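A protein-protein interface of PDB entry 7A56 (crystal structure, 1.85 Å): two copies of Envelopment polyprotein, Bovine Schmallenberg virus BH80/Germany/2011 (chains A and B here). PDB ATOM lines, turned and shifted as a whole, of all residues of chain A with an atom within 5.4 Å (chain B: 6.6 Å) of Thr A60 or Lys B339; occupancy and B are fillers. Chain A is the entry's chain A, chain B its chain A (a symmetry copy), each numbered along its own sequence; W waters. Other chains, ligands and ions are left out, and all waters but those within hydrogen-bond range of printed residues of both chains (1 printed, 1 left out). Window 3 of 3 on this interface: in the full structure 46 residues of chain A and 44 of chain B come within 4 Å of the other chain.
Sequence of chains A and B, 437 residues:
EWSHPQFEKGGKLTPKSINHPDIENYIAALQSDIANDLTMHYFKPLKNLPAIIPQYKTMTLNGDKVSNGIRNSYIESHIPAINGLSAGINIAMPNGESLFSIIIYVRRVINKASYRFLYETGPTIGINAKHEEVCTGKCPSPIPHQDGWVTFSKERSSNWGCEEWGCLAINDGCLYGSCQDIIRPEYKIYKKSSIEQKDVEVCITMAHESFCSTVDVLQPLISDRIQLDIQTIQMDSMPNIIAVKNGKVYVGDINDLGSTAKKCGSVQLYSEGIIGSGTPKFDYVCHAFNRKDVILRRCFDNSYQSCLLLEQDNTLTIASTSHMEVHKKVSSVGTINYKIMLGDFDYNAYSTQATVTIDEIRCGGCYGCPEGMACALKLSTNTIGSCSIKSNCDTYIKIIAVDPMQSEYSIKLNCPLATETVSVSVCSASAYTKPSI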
ATOM      1  N   THR A  58     -29.200 -10.717   3.173  1.00  0.00           N
ATOM      2  CA  THR A  58     -28.528 -10.229   1.965  1.00  0.00           C
ATOM      3  C   THR A  58     -27.307 -11.103   1.689  1.00  0.00           C
ATOM      4  O   THR A  58     -27.172 -12.201   2.228  1.00  0.00           O
ATOM      5  CB  THR A  58     -28.159  -8.739   2.083  1.00  0.00           C
ATOM      6  OG1 THR A  58     -27.717  -8.277   0.801  1.00  0.00           O
ATOM      7  CG2 THR A  58     -27.050  -8.484   3.152  1.00  0.00           C
ATOM      8  N   MET A  59     -26.409 -10.638   0.825  1.00  0.00           N
ATOM      9  CA  MET A  59     -25.296 -11.504   0.459  1.00  0.00           C
ATOM     10  C   MET A  59     -24.331 -11.596   1.628  1.00  0.00           C
ATOM     11  O   MET A  59     -24.326 -10.752   2.518  1.00  0.00           O
ATOM     12  CB  MET A  59     -24.611 -10.977  -0.802  1.00  0.00           C
ATOM     13  CG  MET A  59     -23.598  -9.905  -0.581  1.00  0.00           C
ATOM     14  SD  MET A  59     -24.056  -8.196  -0.644  1.00  0.00           S
ATOM     15  CE  MET A  59     -25.419  -8.022  -1.796  1.00  0.00           C
ATOM     16  N   THR A  60     -23.578 -12.679   1.669  1.00  0.00           N
ATOM     17  CA  THR A  60     -22.623 -12.945   2.740  1.00  0.00           C
ATOM     18  C   THR A  60     -21.274 -13.255   2.120  1.00  0.00           C
ATOM     19  O   THR A  60     -21.186 -13.657   0.955  1.00  0.00           O
ATOM     20  CB  THR A  60     -23.049 -14.110   3.631  1.00  0.00           C
ATOM     21  OG1 THR A  60     -23.090 -15.346   2.853  1.00  0.00           O
ATOM     22  CG2 THR A  60     -24.417 -13.792   4.259  1.00  0.00           C
ATOM     23  N   LEU A  61     -20.219 -13.001   2.883  1.00  0.00           N
ATOM     24  CA  LEU A  61     -18.852 -13.338   2.460  1.00  0.00           C
ATOM     25  C   LEU A  61     -18.323 -14.403   3.393  1.00  0.00           C
ATOM     26  O   LEU A  61     -18.436 -14.260   4.610  1.00  0.00           O
ATOM     27  CB  LEU A  61     -17.957 -12.095   2.516  1.00  0.00           C
ATOM     28  CG  LEU A  61     -18.341 -11.024   1.498  1.00  0.00           C
ATOM     29  CD1 LEU A  61     -17.433  -9.859   1.653  1.00  0.00           C
ATOM     30  CD2 LEU A  61     -18.156 -11.610   0.114  1.00  0.00           C
ATOM     31  N   ASN A  62     -17.742 -15.474   2.847  1.00  0.00           N
ATOM     32  CA  ASN A  62     -17.353 -16.618   3.654  1.00  0.00           C
ATOM     33  C   ASN A  62     -15.856 -16.807   3.439  1.00  0.00           C
ATOM     34  O   ASN A  62     -15.362 -16.552   2.333  1.00  0.00           O
ATOM     35  CB  ASN A  62     -18.208 -17.877   3.243  1.00  0.00           C
ATOM     36  CG  ASN A  62     -19.794 -17.668   3.461  1.00  0.00           C
ATOM     37  OD1 ASN A  62     -20.481 -16.778   2.830  1.00  0.00           O
ATOM     38  ND2 ASN A  62     -20.369 -18.530   4.322  1.00  0.00           N
ATOM     39  N   ILE A  75     -17.960 -15.841   8.574  1.00  0.00           N
ATOM     40  CA  ILE A  75     -18.957 -15.273   7.696  1.00  0.00           C
ATOM     41  C   ILE A  75     -19.062 -13.791   8.043  1.00  0.00           C
ATOM     42  O   ILE A  75     -18.940 -13.388   9.211  1.00  0.00           O
ATOM     43  CB  ILE A  75     -20.325 -15.985   7.818  1.00  0.00           C
ATOM     44  CG1 ILE A  75     -21.309 -15.429   6.772  1.00  0.00           C
ATOM     45  CG2 ILE A  75     -20.885 -15.910   9.245  1.00  0.00           C
ATOM     46  CD1 ILE A  75     -22.480 -16.333   6.509  1.00  0.00           C
ATOM     47  N   GLU A  76     -19.163 -12.985   7.018  1.00  0.00           N
ATOM     48  CA  GLU A  76     -19.307 -11.546   7.189  1.00  0.00           C
ATOM     49  C   GLU A  76     -20.539 -11.084   6.426  1.00  0.00           C
ATOM     50  O   GLU A  76     -20.813 -11.585   5.339  1.00  0.00           O
ATOM     51  CB  GLU A  76     -18.051 -10.848   6.674  1.00  0.00           C
ATOM     52  CG  GLU A  76     -18.002  -9.356   6.983  1.00  0.00           C
ATOM     53  CD  GLU A  76     -18.526  -8.503   5.823  1.00  0.00           C
ATOM     54  OE1 GLU A  76     -18.199  -7.303   5.818  1.00  0.00           O
ATOM     55  OE2 GLU A  76     -19.227  -9.025   4.895  1.00  0.00           O
ATOM     56  N   SER A  77     -21.268 -10.092   6.966  1.00  0.00           N
ATOM     57  CA  SER A  77     -22.389  -9.533   6.213  1.00  0.00           C
ATOM     58  C   SER A  77     -22.702  -8.172   6.840  1.00  0.00           C
ATOM     59  O   SER A  77     -21.907  -7.623   7.621  1.00  0.00           O
ATOM     60  CB  SER A  77     -23.591 -10.484   6.209  1.00  0.00           C
ATOM     61  OG  SER A  77     -24.565 -10.101   5.248  1.00  0.00           O
ATOM     62  N   ILE A  89     -28.293 -16.035  10.958  1.00  0.00           N
ATOM     63  CA  ILE A  89     -27.155 -16.843  10.501  1.00  0.00           C
ATOM     64  C   ILE A  89     -27.306 -18.211  11.095  1.00  0.00           C
ATOM     65  O   ILE A  89     -27.332 -18.359  12.320  1.00  0.00           O
ATOM     66  CB  ILE A  89     -25.786 -16.265  10.887  1.00  0.00           C
ATOM     67  CG1 ILE A  89     -25.638 -14.838  10.361  1.00  0.00           C
ATOM     68  CG2 ILE A  89     -24.619 -17.180  10.351  1.00  0.00           C
ATOM     69  CD1 ILE A  89     -25.272 -14.779   8.883  1.00  0.00           C
ATOM     70  N   ALA A 349     -26.813 -17.448   5.721  1.00  0.00           N
ATOM     71  CA  ALA A 349     -27.859 -16.502   6.116  1.00  0.00           C
ATOM     72  C   ALA A 349     -29.243 -17.113   5.930  1.00  0.00           C
ATOM     73  O   ALA A 349     -29.455 -17.981   5.071  1.00  0.00           O
ATOM     74  CB  ALA A 349     -27.734 -15.224   5.283  1.00  0.00           C
ATOM     75  N   LYS B  65     -16.000 -21.691  -2.706  1.00  0.00           N
ATOM     76  CA  LYS B  65     -16.183 -22.949  -1.977  1.00  0.00           C
ATOM     77  C   LYS B  65     -16.166 -24.094  -2.981  1.00  0.00           C
ATOM     78  O   LYS B  65     -16.707 -23.952  -4.077  1.00  0.00           O
ATOM     79  CB  LYS B  65     -17.519 -23.018  -1.207  1.00  0.00           C
ATOM     80  CG  LYS B  65     -18.135 -21.686  -0.776  1.00  0.00           C
ATOM     81  CD  LYS B  65     -19.381 -21.910   0.099  1.00  0.00           C
ATOM     82  CE  LYS B  65     -19.818 -20.625   0.783  1.00  0.00           C
ATOM     83  NZ  LYS B  65     -20.839 -20.868   1.833  1.00  0.00           N
ATOM     84  N   TYR B  74     -16.777 -16.650  -6.377  1.00  0.00           N
ATOM     85  CA  TYR B  74     -17.571 -15.407  -6.449  1.00  0.00           C
ATOM     86  C   TYR B  74     -16.680 -14.177  -6.501  1.00  0.00           C
ATOM     87  O   TYR B  74     -15.469 -14.199  -6.194  1.00  0.00           O
ATOM     88  CB  TYR B  74     -18.528 -15.276  -5.271  1.00  0.00           C
ATOM     89  CG  TYR B  74     -17.863 -15.109  -3.943  1.00  0.00           C
ATOM     90  CD1 TYR B  74     -17.358 -13.872  -3.531  1.00  0.00           C
ATOM     91  CD2 TYR B  74     -17.769 -16.191  -3.075  1.00  0.00           C
ATOM     92  CE1 TYR B  74     -16.735 -13.731  -2.316  1.00  0.00           C
ATOM     93  CE2 TYR B  74     -17.181 -16.066  -1.846  1.00  0.00           C
ATOM     94  CZ  TYR B  74     -16.668 -14.849  -1.456  1.00  0.00           C
ATOM     95  OH  TYR B  74     -16.083 -14.791  -0.207  1.00  0.00           O
ATOM     96  N   ILE B  75     -17.349 -13.057  -6.830  1.00  0.00           N
ATOM     97  CA  ILE B  75     -16.767 -11.739  -6.716  1.00  0.00           C
ATOM     98  C   ILE B  75     -17.812 -10.846  -6.055  1.00  0.00           C
ATOM     99  O   ILE B  75     -19.025 -10.987  -6.286  1.00  0.00           O
ATOM    100  CB  ILE B  75     -16.316 -11.174  -8.083  1.00  0.00           C
ATOM    101  CG1 ILE B  75     -15.586  -9.831  -7.888  1.00  0.00           C
ATOM    102  CG2 ILE B  75     -17.484 -11.065  -9.072  1.00  0.00           C
ATOM    103  CD1 ILE B  75     -14.737  -9.433  -9.061  1.00  0.00           C
ATOM    104  N   GLU B  76     -17.350 -10.023  -5.151  1.00  0.00           N
ATOM    105  CA  GLU B  76     -18.220  -9.081  -4.458  1.00  0.00           C
ATOM    106  C   GLU B  76     -17.648  -7.682  -4.613  1.00  0.00           C
ATOM    107  O   GLU B  76     -16.433  -7.506  -4.577  1.00  0.00           O
ATOM    108  CB  GLU B  76     -18.317  -9.473  -2.986  1.00  0.00           C
ATOM    109  CG  GLU B  76     -19.357  -8.681  -2.203  1.00  0.00           C
ATOM    110  CD  GLU B  76     -18.747  -7.476  -1.479  1.00  0.00           C
ATOM    111  OE1 GLU B  76     -19.408  -6.991  -0.543  1.00  0.00           O
ATOM    112  OE2 GLU B  76     -17.598  -7.032  -1.806  1.00  0.00           O
ATOM    113  N   SER B  77     -18.518  -6.665  -4.741  1.00  0.00           N
ATOM    114  CA  SER B  77     -18.019  -5.292  -4.770  1.00  0.00           C
ATOM    115  C   SER B  77     -19.211  -4.386  -4.450  1.00  0.00           C
ATOM    116  O   SER B  77     -20.262  -4.847  -3.976  1.00  0.00           O
ATOM    117  CB  SER B  77     -17.360  -4.964  -6.115  1.00  0.00           C
ATOM    118  OG  SER B  77     -16.614  -3.755  -6.057  1.00  0.00           O
ATOM    119  N   ARG B 225     -27.620 -16.709  -8.518  1.00  0.00           N
ATOM    120  CA  ARG B 225     -26.259 -16.307  -8.871  1.00  0.00           C
ATOM    121  C   ARG B 225     -25.885 -14.895  -8.431  1.00  0.00           C
ATOM    122  O   ARG B 225     -24.687 -14.614  -8.190  1.00  0.00           O
ATOM    123  CB  ARG B 225     -26.099 -16.403 -10.391  1.00  0.00           C
ATOM    124  CG  ARG B 225     -26.178 -17.854 -10.900  1.00  0.00           C
ATOM    125  CD  ARG B 225     -26.520 -17.871 -12.383  1.00  0.00           C
ATOM    126  NE  ARG B 225     -26.535 -19.244 -12.851  1.00  0.00           N
ATOM    127  CZ  ARG B 225     -27.556 -20.079 -12.677  1.00  0.00           C
ATOM    128  NH1 ARG B 225     -28.660 -19.661 -12.084  1.00  0.00           N
ATOM    129  NH2 ARG B 225     -27.466 -21.349 -13.116  1.00  0.00           N
ATOM    130  N   ILE B 226     -26.852 -13.978  -8.354  1.00  0.00           N
ATOM    131  CA  ILE B 226     -26.524 -12.569  -8.124  1.00  0.00           C
ATOM    132  C   ILE B 226     -27.398 -11.993  -7.024  1.00  0.00           C
ATOM    133  O   ILE B 226     -28.629 -12.149  -7.034  1.00  0.00           O
ATOM    134  CB  ILE B 226     -26.657 -11.725  -9.404  1.00  0.00           C
ATOM    135  CG1 ILE B 226     -25.780 -12.314 -10.545  1.00  0.00           C
ATOM    136  CG2 ILE B 226     -26.363 -10.211  -9.073  1.00  0.00           C
ATOM    137  CD1 ILE B 226     -26.140 -11.666 -11.897  1.00  0.00           C
ATOM    138  N   GLN B 227     -26.758 -11.390  -6.032  1.00  0.00           N
ATOM    139  CA  GLN B 227     -27.510 -10.687  -4.998  1.00  0.00           C
ATOM    140  C   GLN B 227     -27.107  -9.220  -4.984  1.00  0.00           C
ATOM    141  O   GLN B 227     -25.932  -8.884  -5.178  1.00  0.00           O
ATOM    142  CB  GLN B 227     -27.269 -11.334  -3.601  1.00  0.00           C
ATOM    143  CG  GLN B 227     -27.752 -12.771  -3.488  1.00  0.00           C
ATOM    144  CD  GLN B 227     -26.699 -13.677  -3.766  1.00  0.00           C
ATOM    145  OE1 GLN B 227     -25.600 -13.552  -3.192  1.00  0.00           O
ATOM    146  NE2 GLN B 227     -26.971 -14.650  -4.675  1.00  0.00           N
ATOM    147  N   LEU B 228     -28.079  -8.331  -4.717  1.00  0.00           N
ATOM    148  CA  LEU B 228     -27.752  -6.928  -4.581  1.00  0.00           C
ATOM    149  C   LEU B 228     -28.552  -6.343  -3.420  1.00  0.00           C
ATOM    150  O   LEU B 228     -29.634  -6.833  -3.094  1.00  0.00           O
ATOM    151  CB  LEU B 228     -28.082  -6.106  -5.862  1.00  0.00           C
ATOM    152  CG  LEU B 228     -27.578  -6.591  -7.237  1.00  0.00           C
ATOM    153  CD1 LEU B 228     -28.694  -7.422  -7.830  1.00  0.00           C
ATOM    154  CD2 LEU B 228     -27.213  -5.399  -8.141  1.00  0.00           C
ATOM    155  N   ASN B 337     -24.498  -2.788  -2.830  1.00  0.00           N
ATOM    156  CA  ASN B 337     -23.604  -3.944  -2.730  1.00  0.00           C
ATOM    157  C   ASN B 337     -24.065  -5.019  -3.690  1.00  0.00           C
ATOM    158  O   ASN B 337     -25.272  -5.161  -3.931  1.00  0.00           O
ATOM    159  CB  ASN B 337     -23.598  -4.456  -1.284  1.00  0.00           C
ATOM    160  CG  ASN B 337     -23.086  -3.428  -0.336  1.00  0.00           C
ATOM    161  OD1 ASN B 337     -21.921  -3.076  -0.395  1.00  0.00           O
ATOM    162  ND2 ASN B 337     -23.949  -2.892   0.522  1.00  0.00           N
ATOM    163  N   TYR B 338     -23.107  -5.798  -4.239  1.00  0.00           N
ATOM    164  CA  TYR B 338     -23.517  -6.875  -5.116  1.00  0.00           C
ATOM    165  C   TYR B 338     -22.500  -8.015  -5.043  1.00  0.00           C
ATOM    166  O   TYR B 338     -21.309  -7.795  -4.803  1.00  0.00           O
ATOM    167  CB  TYR B 338     -23.647  -6.432  -6.583  1.00  0.00           C
ATOM    168  CG  TYR B 338     -22.405  -5.739  -7.194  1.00  0.00           C
ATOM    169  CD1 TYR B 338     -21.416  -6.497  -7.817  1.00  0.00           C
ATOM    170  CD2 TYR B 338     -22.245  -4.353  -7.160  1.00  0.00           C
ATOM    171  CE1 TYR B 338     -20.306  -5.910  -8.402  1.00  0.00           C
ATOM    172  CE2 TYR B 338     -21.127  -3.715  -7.765  1.00  0.00           C
ATOM    173  CZ  TYR B 338     -20.140  -4.552  -8.383  1.00  0.00           C
ATOM    174  OH  TYR B 338     -19.034  -3.994  -9.011  1.00  0.00           O
ATOM    175  N   LYS B 339     -23.007  -9.213  -5.286  1.00  0.00           N
ATOM    176  CA  LYS B 339     -22.210 -10.436  -5.295  1.00  0.00           C
ATOM    177  C   LYS B 339     -22.669 -11.304  -6.452  1.00  0.00           C
ATOM    178  O   LYS B 339     -23.877 -11.513  -6.660  1.00  0.00           O
ATOM    179  CB  LYS B 339     -22.341 -11.160  -3.936  1.00  0.00           C
ATOM    180  CG  LYS B 339     -21.440 -12.481  -3.805  1.00  0.00           C
ATOM    181  CD  LYS B 339     -21.908 -13.283  -2.612  1.00  0.00           C
ATOM    182  CE  LYS B 339     -21.013 -14.633  -2.447  1.00  0.00           C
ATOM    183  NZ  LYS B 339     -21.426 -15.337  -1.189  1.00  0.00           N
ATOM    184  N   ILE B 340     -21.684 -11.817  -7.208  1.00  0.00           N
ATOM    185  CA  ILE B 340     -21.912 -12.627  -8.407  1.00  0.00           C
ATOM    186  C   ILE B 340     -21.150 -13.944  -8.224  1.00  0.00           C
ATOM    187  O   ILE B 340     -19.968 -13.924  -7.858  1.00  0.00           O
ATOM    188  CB  ILE B 340     -21.411 -11.907  -9.675  1.00  0.00           C
ATOM    189  CG1 ILE B 340     -22.199 -10.600  -9.934  1.00  0.00           C
ATOM    190  CG2 ILE B 340     -21.432 -12.858 -10.907  1.00  0.00           C
ATOM    191  CD1 ILE B 340     -21.321  -9.596 -10.727  1.00  0.00           C
ATOM    192  N   MET B 341     -21.868 -15.063  -8.363  1.00  0.00           N
ATOM    193  CA  MET B 341     -21.333 -16.434  -8.180  1.00  0.00           C
ATOM    194  C   MET B 341     -21.884 -17.310  -9.293  1.00  0.00           C
ATOM    195  O   MET B 341     -23.021 -17.796  -9.192  1.00  0.00           O
ATOM    196  CB  MET B 341     -21.750 -16.957  -6.811  1.00  0.00           C
ATOM    197  CG  MET B 341     -21.177 -18.388  -6.441  1.00  0.00           C
ATOM    198  SD  MET B 341     -21.185 -18.474  -4.630  1.00  0.00           S
ATOM    199  CE  MET B 341     -19.755 -19.533  -4.347  1.00  0.00           C
HETATM  200  O   HOH W   1     -24.497 -14.640  -0.546  1.00  0.00           O
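The side-chain amino group (NZ) of Lys B339 lies within hydrogen-bond range of the backbone carbonyl oxygen (O) of Thr A60 (2.7 Å). NZ of Lys B65 lies close to ND2 of Asn A62, 3.4 Å away. The side-chain hydroxyl (OH) of Tyr B74 sits at hydrogen-bond distance from the backbone carbonyl oxygen (O) of Asn A62 (3.2 Å).
O of Met A59 is in hydrogen-bond range of OG of Ser A77, at 2.8 Å. The side-chain hydroxyl (OG1) of Thr A60 is in hydrogen-bond range of the side-chain amide oxygen (OD1) of Asn A62. The backbone carbonyl oxygen (O) of Leu A61 sits at hydrogen-bond distance from the backbone NH (N) of Glu A76, 2.8 Å away. The backbone carbonyl oxygen of Ser B77 is in hydrogen-bond range of the backbone NH of Tyr B338, at 3.0 Å. N of Lys B339 is in hydrogen-bond range of O of Gln B227 (2.9 Å).
Among the printed residues, merely in contact across the chains: Leu A61 with Tyr B74 (3.5 Å), Met A59 with Gln B227 (3.5 Å), Met A59 with Asn B337 (3.6 Å), Leu A61 with Glu B76 (3.8 Å), Met A59 with Leu B228 (3.8 Å), Met A59 with Lys B339 (3.8 Å) and Met A59 with Tyr B338 (3.99 Å).
Thr A60 touches just one residue of chain B: Lys B339. Of the printed residues of chain B, Asn A62 touches Lys B65 and Tyr B74. Ser B77 touches none of the printed residues of chain A. Of the printed residues of chain A, Leu B228 touches Met A59 (3.8 Å). Of the printed residues of chain A, Asn B337 touches Met A59. The nearest residue of chain B that does not touch Thr A60 is Tyr B74 (5.3 Å). The nearest residue of chain A that does not touch Lys B339 is Asn A62 (4.4 Å). The nearest printed residue of chain A that does not touch Tyr B338 is Leu A61 (7.0 Å).
Printed residues of chain A that touch a printed residue of chain B: Met A59, Thr A60, Leu A61 and Asn A62. Hydrophobic or aromatic side chains of chain A that line the printed part of chain B: Met A59 and Leu A61. Along chain A the printed residues that touch a printed residue of chain B span positions 59 to 62. Of the 14 printed residues of chain B, 8 touch a printed residue of chain A. Hydrophobic or aromatic side chains of chain B within 4 Å of the printed part of chain A: Tyr B74.
Positions printed for both chains: 75, 76 and 77.
Water W1 lies within hydrogen-bond range of OE1 of Gln B227, N of Thr A60 and NZ of Lys B339.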
